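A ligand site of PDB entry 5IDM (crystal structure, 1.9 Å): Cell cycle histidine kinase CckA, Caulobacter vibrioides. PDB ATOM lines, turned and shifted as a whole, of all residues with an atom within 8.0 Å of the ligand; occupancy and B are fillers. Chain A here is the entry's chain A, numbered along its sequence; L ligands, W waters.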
ATOM      1  N   GLY A  87     -23.339   7.163   1.436  1.00  0.00           N
ATOM      2  CA  GLY A  87     -22.964   7.366   0.022  1.00  0.00           C
ATOM      3  C   GLY A  87     -21.670   8.090  -0.259  1.00  0.00           C
ATOM      4  O   GLY A  87     -21.524   8.679  -1.320  1.00  0.00           O
ATOM      5  N   PHE A  88     -20.692   7.983   0.653  1.00  0.00           N
ATOM      6  CA  PHE A  88     -19.337   8.525   0.461  1.00  0.00           C
ATOM      7  C   PHE A  88     -18.354   7.345   0.485  1.00  0.00           C
ATOM      8  O   PHE A  88     -17.834   7.009   1.551  1.00  0.00           O
ATOM      9  CB  PHE A  88     -19.034   9.550   1.553  1.00  0.00           C
ATOM     10  CG  PHE A  88     -17.647  10.180   1.478  1.00  0.00           C
ATOM     11  CD1 PHE A  88     -16.931  10.299   0.285  1.00  0.00           C
ATOM     12  CD2 PHE A  88     -17.064  10.674   2.648  1.00  0.00           C
ATOM     13  CE1 PHE A  88     -15.661  10.877   0.266  1.00  0.00           C
ATOM     14  CE2 PHE A  88     -15.806  11.260   2.629  1.00  0.00           C
ATOM     15  CZ  PHE A  88     -15.106  11.365   1.441  1.00  0.00           C
ATOM     16  N   PRO A  89     -18.122   6.721  -0.681  1.00  0.00           N
ATOM     17  CA  PRO A  89     -17.339   5.467  -0.711  1.00  0.00           C
ATOM     18  C   PRO A  89     -15.907   5.587  -0.172  1.00  0.00           C
ATOM     19  O   PRO A  89     -15.428   4.653   0.453  1.00  0.00           O
ATOM     20  CB  PRO A  89     -17.319   5.065  -2.181  1.00  0.00           C
ATOM     21  CG  PRO A  89     -18.278   5.946  -2.898  1.00  0.00           C
ATOM     22  CD  PRO A  89     -18.681   7.065  -2.000  1.00  0.00           C
ATOM     23  N   PHE A 116     -26.813  17.886 -12.025  1.00  0.00           N
ATOM     24  CA  PHE A 116     -25.677  18.776 -11.761  1.00  0.00           C
ATOM     25  C   PHE A 116     -25.172  19.521 -13.001  1.00  0.00           C
ATOM     26  O   PHE A 116     -24.283  20.355 -12.896  1.00  0.00           O
ATOM     27  CB  PHE A 116     -24.533  17.987 -11.122  1.00  0.00           C
ATOM     28  CG  PHE A 116     -24.855  17.513  -9.736  1.00  0.00           C
ATOM     29  CD1 PHE A 116     -24.955  18.423  -8.696  1.00  0.00           C
ATOM     30  CD2 PHE A 116     -25.064  16.165  -9.477  1.00  0.00           C
ATOM     31  CE1 PHE A 116     -25.249  18.007  -7.414  1.00  0.00           C
ATOM     32  CE2 PHE A 116     -25.362  15.742  -8.188  1.00  0.00           C
ATOM     33  CZ  PHE A 116     -25.456  16.673  -7.154  1.00  0.00           C
ATOM     34  N   TYR A 137     -22.402  21.717  -6.681  1.00  0.00           N
ATOM     35  CA  TYR A 137     -21.363  20.733  -6.993  1.00  0.00           C
ATOM     36  C   TYR A 137     -19.962  21.332  -6.952  1.00  0.00           C
ATOM     37  O   TYR A 137     -19.059  20.809  -6.315  1.00  0.00           O
ATOM     38  CB  TYR A 137     -21.605  20.093  -8.342  1.00  0.00           C
ATOM     39  CG  TYR A 137     -20.799  18.849  -8.574  1.00  0.00           C
ATOM     40  CD1 TYR A 137     -21.232  17.620  -8.095  1.00  0.00           C
ATOM     41  CD2 TYR A 137     -19.615  18.893  -9.292  1.00  0.00           C
ATOM     42  CE1 TYR A 137     -20.513  16.465  -8.320  1.00  0.00           C
ATOM     43  CE2 TYR A 137     -18.879  17.738  -9.523  1.00  0.00           C
ATOM     44  CZ  TYR A 137     -19.336  16.538  -9.026  1.00  0.00           C
ATOM     45  OH  TYR A 137     -18.661  15.378  -9.240  1.00  0.00           O
ATOM     46  N   VAL A 140     -18.886  22.155  -3.318  1.00  0.00           N
ATOM     47  CA  VAL A 140     -18.539  20.934  -2.583  1.00  0.00           C
ATOM     48  C   VAL A 140     -17.136  20.465  -2.963  1.00  0.00           C
ATOM     49  O   VAL A 140     -16.322  20.182  -2.079  1.00  0.00           O
ATOM     50  CB  VAL A 140     -19.564  19.798  -2.834  1.00  0.00           C
ATOM     51  CG1 VAL A 140     -19.087  18.467  -2.239  1.00  0.00           C
ATOM     52  CG2 VAL A 140     -20.923  20.176  -2.265  1.00  0.00           C
ATOM     53  N   LYS A 141     -16.823  20.428  -4.261  1.00  0.00           N
ATOM     54  CA  LYS A 141     -15.486  20.013  -4.698  1.00  0.00           C
ATOM     55  C   LYS A 141     -14.380  21.000  -4.265  1.00  0.00           C
ATOM     56  O   LYS A 141     -13.295  20.580  -3.855  1.00  0.00           O
ATOM     57  CB  LYS A 141     -15.444  19.738  -6.204  1.00  0.00           C
ATOM     58  CG  LYS A 141     -16.458  18.699  -6.718  1.00  0.00           C
ATOM     59  CD  LYS A 141     -16.553  17.419  -5.908  1.00  0.00           C
ATOM     60  CE  LYS A 141     -15.258  16.608  -5.908  1.00  0.00           C
ATOM     61  NZ  LYS A 141     -15.461  15.369  -5.133  1.00  0.00           N
ATOM     62  N   ASP A 144     -13.106  20.353  -0.843  1.00  0.00           N
ATOM     63  CA  ASP A 144     -12.528  19.013  -0.733  1.00  0.00           C
ATOM     64  C   ASP A 144     -13.536  17.988  -0.242  1.00  0.00           C
ATOM     65  O   ASP A 144     -13.189  17.058   0.498  1.00  0.00           O
ATOM     66  CB  ASP A 144     -11.267  19.021   0.155  1.00  0.00           C
ATOM     67  CG  ASP A 144     -10.182  19.930  -0.384  1.00  0.00           C
ATOM     68  OD1 ASP A 144      -9.965  19.938  -1.612  1.00  0.00           O
ATOM     69  OD2 ASP A 144      -9.518  20.618   0.432  1.00  0.00           O
ATOM     70  N   GLY A 145     -14.775  18.169  -0.681  1.00  0.00           N
ATOM     71  CA  GLY A 145     -15.888  17.348  -0.233  1.00  0.00           C
ATOM     72  C   GLY A 145     -16.432  16.404  -1.290  1.00  0.00           C
ATOM     73  O   GLY A 145     -15.894  16.296  -2.409  1.00  0.00           O
ATOM     74  N   TRP A 146     -17.500  15.731  -0.908  1.00  0.00           N
ATOM     75  CA  TRP A 146     -18.202  14.762  -1.748  1.00  0.00           C
ATOM     76  C   TRP A 146     -19.696  15.013  -1.569  1.00  0.00           C
ATOM     77  O   TRP A 146     -20.147  15.309  -0.470  1.00  0.00           O
ATOM     78  CB  TRP A 146     -17.863  13.349  -1.277  1.00  0.00           C
ATOM     79  CG  TRP A 146     -18.445  12.240  -2.142  1.00  0.00           C
ATOM     80  CD1 TRP A 146     -19.629  11.597  -1.939  1.00  0.00           C
ATOM     81  CD2 TRP A 146     -17.857  11.635  -3.304  1.00  0.00           C
ATOM     82  NE1 TRP A 146     -19.826  10.657  -2.930  1.00  0.00           N
ATOM     83  CE2 TRP A 146     -18.738  10.645  -3.759  1.00  0.00           C
ATOM     84  CE3 TRP A 146     -16.645  11.825  -3.978  1.00  0.00           C
ATOM     85  CZ2 TRP A 146     -18.465   9.848  -4.893  1.00  0.00           C
ATOM     86  CZ3 TRP A 146     -16.372  11.043  -5.112  1.00  0.00           C
ATOM     87  CH2 TRP A 146     -17.273  10.061  -5.555  1.00  0.00           C
ATOM     88  N   ILE A 147     -20.454  14.887  -2.652  1.00  0.00           N
ATOM     89  CA  ILE A 147     -21.907  15.031  -2.574  1.00  0.00           C
ATOM     90  C   ILE A 147     -22.559  13.771  -3.148  1.00  0.00           C
ATOM     91  O   ILE A 147     -22.143  13.263  -4.200  1.00  0.00           O
ATOM     92  CB  ILE A 147     -22.418  16.322  -3.245  1.00  0.00           C
ATOM     93  CG1 ILE A 147     -23.935  16.420  -3.151  1.00  0.00           C
ATOM     94  CG2 ILE A 147     -21.928  16.442  -4.688  1.00  0.00           C
ATOM     95  CD1 ILE A 147     -24.464  17.836  -3.305  1.00  0.00           C
ATOM     96  N   HIS A 148     -23.529  13.249  -2.427  1.00  0.00           N
ATOM     97  CA  HIS A 148     -24.284  12.076  -2.849  1.00  0.00           C
ATOM     98  C   HIS A 148     -25.768  12.421  -2.813  1.00  0.00           C
ATOM     99  O   HIS A 148     -26.222  13.067  -1.868  1.00  0.00           O
ATOM    100  CB  HIS A 148     -24.035  10.898  -1.924  1.00  0.00           C
ATOM    101  CG  HIS A 148     -24.802   9.667  -2.302  1.00  0.00           C
ATOM    102  ND1 HIS A 148     -24.359   8.781  -3.252  1.00  0.00           N
ATOM    103  CD2 HIS A 148     -26.004   9.205  -1.887  1.00  0.00           C
ATOM    104  CE1 HIS A 148     -25.250   7.813  -3.400  1.00  0.00           C
ATOM    105  NE2 HIS A 148     -26.258   8.042  -2.577  1.00  0.00           N
ATOM    106  N   VAL A 149     -26.506  11.959  -3.816  1.00  0.00           N
ATOM    107  CA  VAL A 149     -27.949  12.212  -3.880  1.00  0.00           C
ATOM    108  C   VAL A 149     -28.675  10.884  -3.722  1.00  0.00           C
ATOM    109  O   VAL A 149     -28.396   9.937  -4.449  1.00  0.00           O
ATOM    110  CB  VAL A 149     -28.346  12.888  -5.192  1.00  0.00           C
ATOM    111  CG1 VAL A 149     -29.810  13.303  -5.160  1.00  0.00           C
ATOM    112  CG2 VAL A 149     -27.462  14.084  -5.461  1.00  0.00           C
ATOM    113  N   ARG A 160     -26.665  15.070   0.190  1.00  0.00           N
ATOM    114  CA  ARG A 160     -25.766  14.813   1.301  1.00  0.00           C
ATOM    115  C   ARG A 160     -24.370  15.328   0.982  1.00  0.00           C
ATOM    116  O   ARG A 160     -23.756  14.866   0.018  1.00  0.00           O
ATOM    117  CB  ARG A 160     -25.707  13.319   1.537  1.00  0.00           C
ATOM    118  CG  ARG A 160     -27.033  12.741   2.028  1.00  0.00           C
ATOM    119  CD  ARG A 160     -26.998  11.224   2.038  1.00  0.00           C
ATOM    120  NE  ARG A 160     -28.290  10.661   2.398  1.00  0.00           N
ATOM    121  CZ  ARG A 160     -28.639   9.385   2.225  1.00  0.00           C
ATOM    122  NH1 ARG A 160     -27.794   8.507   1.677  1.00  0.00           N
ATOM    123  NH2 ARG A 160     -29.855   8.967   2.594  1.00  0.00           N
ATOM    124  N   ILE A 161     -23.881  16.280   1.773  1.00  0.00           N
ATOM    125  CA  ILE A 161     -22.542  16.836   1.621  1.00  0.00           C
ATOM    126  C   ILE A 161     -21.640  16.268   2.720  1.00  0.00           C
ATOM    127  O   ILE A 161     -22.002  16.311   3.896  1.00  0.00           O
ATOM    128  CB  ILE A 161     -22.564  18.373   1.664  1.00  0.00           C
ATOM    129  CG1 ILE A 161     -23.319  18.908   0.445  1.00  0.00           C
ATOM    130  CG2 ILE A 161     -21.136  18.935   1.733  1.00  0.00           C
ATOM    131  CD1 ILE A 161     -23.643  20.380   0.524  1.00  0.00           C
ATOM    132  N   PHE A 162     -20.503  15.714   2.308  1.00  0.00           N
ATOM    133  CA  PHE A 162     -19.543  15.133   3.222  1.00  0.00           C
ATOM    134  C   PHE A 162     -18.293  15.982   3.133  1.00  0.00           C
ATOM    135  O   PHE A 162     -17.754  16.164   2.038  1.00  0.00           O
ATOM    136  CB  PHE A 162     -19.216  13.695   2.831  1.00  0.00           C
ATOM    137  CG  PHE A 162     -20.410  12.790   2.751  1.00  0.00           C
ATOM    138  CD1 PHE A 162     -21.134  12.693   1.571  1.00  0.00           C
ATOM    139  CD2 PHE A 162     -20.809  12.029   3.841  1.00  0.00           C
ATOM    140  CE1 PHE A 162     -22.232  11.847   1.482  1.00  0.00           C
ATOM    141  CE2 PHE A 162     -21.907  11.183   3.752  1.00  0.00           C
ATOM    142  CZ  PHE A 162     -22.615  11.085   2.566  1.00  0.00           C
HETATM  143  P1  LIG L   1     -12.132  13.499  -9.891  1.00  0.00           P
HETATM  144  O1  LIG L   1     -12.421  14.837  -9.254  1.00  0.00           O
HETATM  145  O2  LIG L   1     -11.122  12.555  -9.319  1.00  0.00           O
HETATM  146  O3  LIG L   1     -13.533  12.731  -9.999  1.00  0.00           O
HETATM  147  C1  LIG L   1     -13.616  11.467 -10.643  1.00  0.00           C
HETATM  148  C2  LIG L   1     -15.070  11.035 -10.767  1.00  0.00           C
HETATM  149  O4  LIG L   1     -15.671  10.796  -9.489  1.00  0.00           O
HETATM  150  C3  LIG L   1     -15.957  12.082 -11.434  1.00  0.00           C
HETATM  151  O5  LIG L   1     -15.864  12.029 -12.838  1.00  0.00           O
HETATM  152  C4  LIG L   1     -17.334  11.712 -10.956  1.00  0.00           C
HETATM  153  O6  LIG L   1     -17.912  10.622 -11.705  1.00  0.00           O
HETATM  154  C5  LIG L   1     -17.039  11.244  -9.554  1.00  0.00           C
HETATM  155  N1  LIG L   1     -17.186  12.263  -8.507  1.00  0.00           N
HETATM  156  C6  LIG L   1     -16.223  13.093  -8.026  1.00  0.00           C
HETATM  157  N2  LIG L   1     -16.705  13.838  -7.016  1.00  0.00           N
HETATM  158  C7  LIG L   1     -17.995  13.463  -6.831  1.00  0.00           C
HETATM  159  C8  LIG L   1     -19.072  13.834  -5.902  1.00  0.00           C
HETATM  160  O7  LIG L   1     -18.864  14.713  -5.051  1.00  0.00           O
HETATM  161  N3  LIG L   1     -20.261  13.213  -6.017  1.00  0.00           N
HETATM  162  C9  LIG L   1     -20.499  12.259  -6.950  1.00  0.00           C
HETATM  163  N4  LIG L   1     -21.712  11.680  -7.012  1.00  0.00           N
HETATM  164  N5  LIG L   1     -19.536  11.857  -7.829  1.00  0.00           N
HETATM  165  C10 LIG L   1     -18.304  12.414  -7.796  1.00  0.00           C
HETATM  166  P2  LIG L   1     -16.131  13.348 -13.708  1.00  0.00           P
HETATM  167  O8  LIG L   1     -17.226  14.150 -13.025  1.00  0.00           O
HETATM  168  O9  LIG L   1     -16.358  12.836 -15.118  1.00  0.00           O
HETATM  169  O10 LIG L   1     -14.760  14.173 -13.588  1.00  0.00           O
HETATM  170  C11 LIG L   1     -13.557  13.617 -14.075  1.00  0.00           C
HETATM  171  C12 LIG L   1     -12.372  14.452 -13.645  1.00  0.00           C
HETATM  172  O11 LIG L   1     -12.394  15.719 -14.295  1.00  0.00           O
HETATM  173  C13 LIG L   1     -12.318  14.787 -12.165  1.00  0.00           C
HETATM  174  O12 LIG L   1     -11.736  13.711 -11.437  1.00  0.00           O
HETATM  175  C14 LIG L   1     -11.473  16.050 -12.150  1.00  0.00           C
HETATM  176  O13 LIG L   1     -10.100  15.715 -12.100  1.00  0.00           O
HETATM  177  C15 LIG L   1     -11.684  16.675 -13.502  1.00  0.00           C
HETATM  178  N6  LIG L   1     -12.563  17.859 -13.618  1.00  0.00           N
HETATM  179  C16 LIG L   1     -13.849  17.961 -13.227  1.00  0.00           C
HETATM  180  N7  LIG L   1     -14.362  19.167 -13.559  1.00  0.00           N
HETATM  181  C17 LIG L   1     -13.390  19.835 -14.202  1.00  0.00           C
HETATM  182  C18 LIG L   1     -13.245  21.166 -14.820  1.00  0.00           C
HETATM  183  O14 LIG L   1     -14.218  21.955 -14.823  1.00  0.00           O
HETATM  184  N8  LIG L   1     -12.054  21.482 -15.370  1.00  0.00           N
HETATM  185  C19 LIG L   1     -10.998  20.639 -15.368  1.00  0.00           C
HETATM  186  N9  LIG L   1      -9.836  21.015 -15.940  1.00  0.00           N
HETATM  187  N10 LIG L   1     -11.057  19.391 -14.793  1.00  0.00           N
HETATM  188  C20 LIG L   1     -12.200  18.966 -14.233  1.00  0.00           C
HETATM  189  O   HOH W   1     -12.866  14.342  -6.225  1.00  0.00           O
HETATM  190  O   HOH W   2     -19.591   8.948  -8.431  1.00  0.00           O
HETATM  191  O   HOH W   3     -24.726  11.073  -6.095  1.00  0.00           O
HETATM  192  O   HOH W   4     -22.600  10.300  -9.138  1.00  0.00           O
HETATM  193  O   HOH W   5     -10.982  10.714  -7.236  1.00  0.00           O
HETATM  194  O   HOH W   6      -9.256  11.508 -10.874  1.00  0.00           O
HETATM  195  O   HOH W   7     -20.393  10.076 -11.181  1.00  0.00           O
HETATM  196  O   HOH W   8     -16.956   7.836 -11.009  1.00  0.00           O
HETATM  197  O   HOH W   9     -14.309   9.026  -7.418  1.00  0.00           O
HETATM  198  O   HOH W  10     -10.636  22.333 -12.501  1.00  0.00           O
HETATM  199  O   HOH W  11     -17.873  10.587 -14.575  1.00  0.00           O
HETATM  200  O   HOH W  12      -8.404  18.297 -12.762  1.00  0.00           O
HETATM  201  O   HOH W  13      -7.354  19.691 -15.081  1.00  0.00           O
HETATM  202  O   HOH W  14     -16.603  15.572 -10.647  1.00  0.00           O
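The backbone NH of Phe 162 sits at hydrogen-bond distance from the backbone carbonyl oxygen of Trp 146 (2.8 Å).
The side-chain amino group (NZ) of Lys 141 is in hydrogen-bond range of the backbone carbonyl oxygen (O) of Gly 145, at 2.9 Å.
The indole nitrogen (NE1) of Trp 146 is in hydrogen-bond range of the backbone carbonyl oxygen (O) of Gly 87 (3.1 Å).
A nitrogen (N2) of the ligand sits close to the side-chain hydroxyl (OH) of Tyr 137, 3.3 Å away.
The backbone NH of Ile 147 lies within hydrogen-bond range of an oxygen (O7) of the ligand, 2.9 Å away.
O of Ile 147 lies within hydrogen-bond range of N3 of the ligand, at 2.6 Å.
NZ of Lys 141 sits at hydrogen-bond distance from N2 of the ligand (2.7 Å).
Residues that only touch the ligand: Trp 146.
Hydrophobic or aromatic side chains within 4 Å of the ligand: Tyr 137, Trp 146 and Ile 147.
Of the 16 residues printed, 4 come within 4 Å of the ligand.
Along chain A the residues within 4 Å of the ligand span positions 137 to 147.
Water W14 bridges the side-chain hydroxyl (OH) of Tyr 137 (2.5 Å) and an oxygen (O8) of the ligand (2.8 Å).
Water W1 bridges NZ of Lys 141 (3.0 Å) and O1 of the ligand (3.1 Å).
Water W3 lies within hydrogen-bond range of N of Val 149 (3.0 Å) and N4 of the ligand (3.2 Å).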
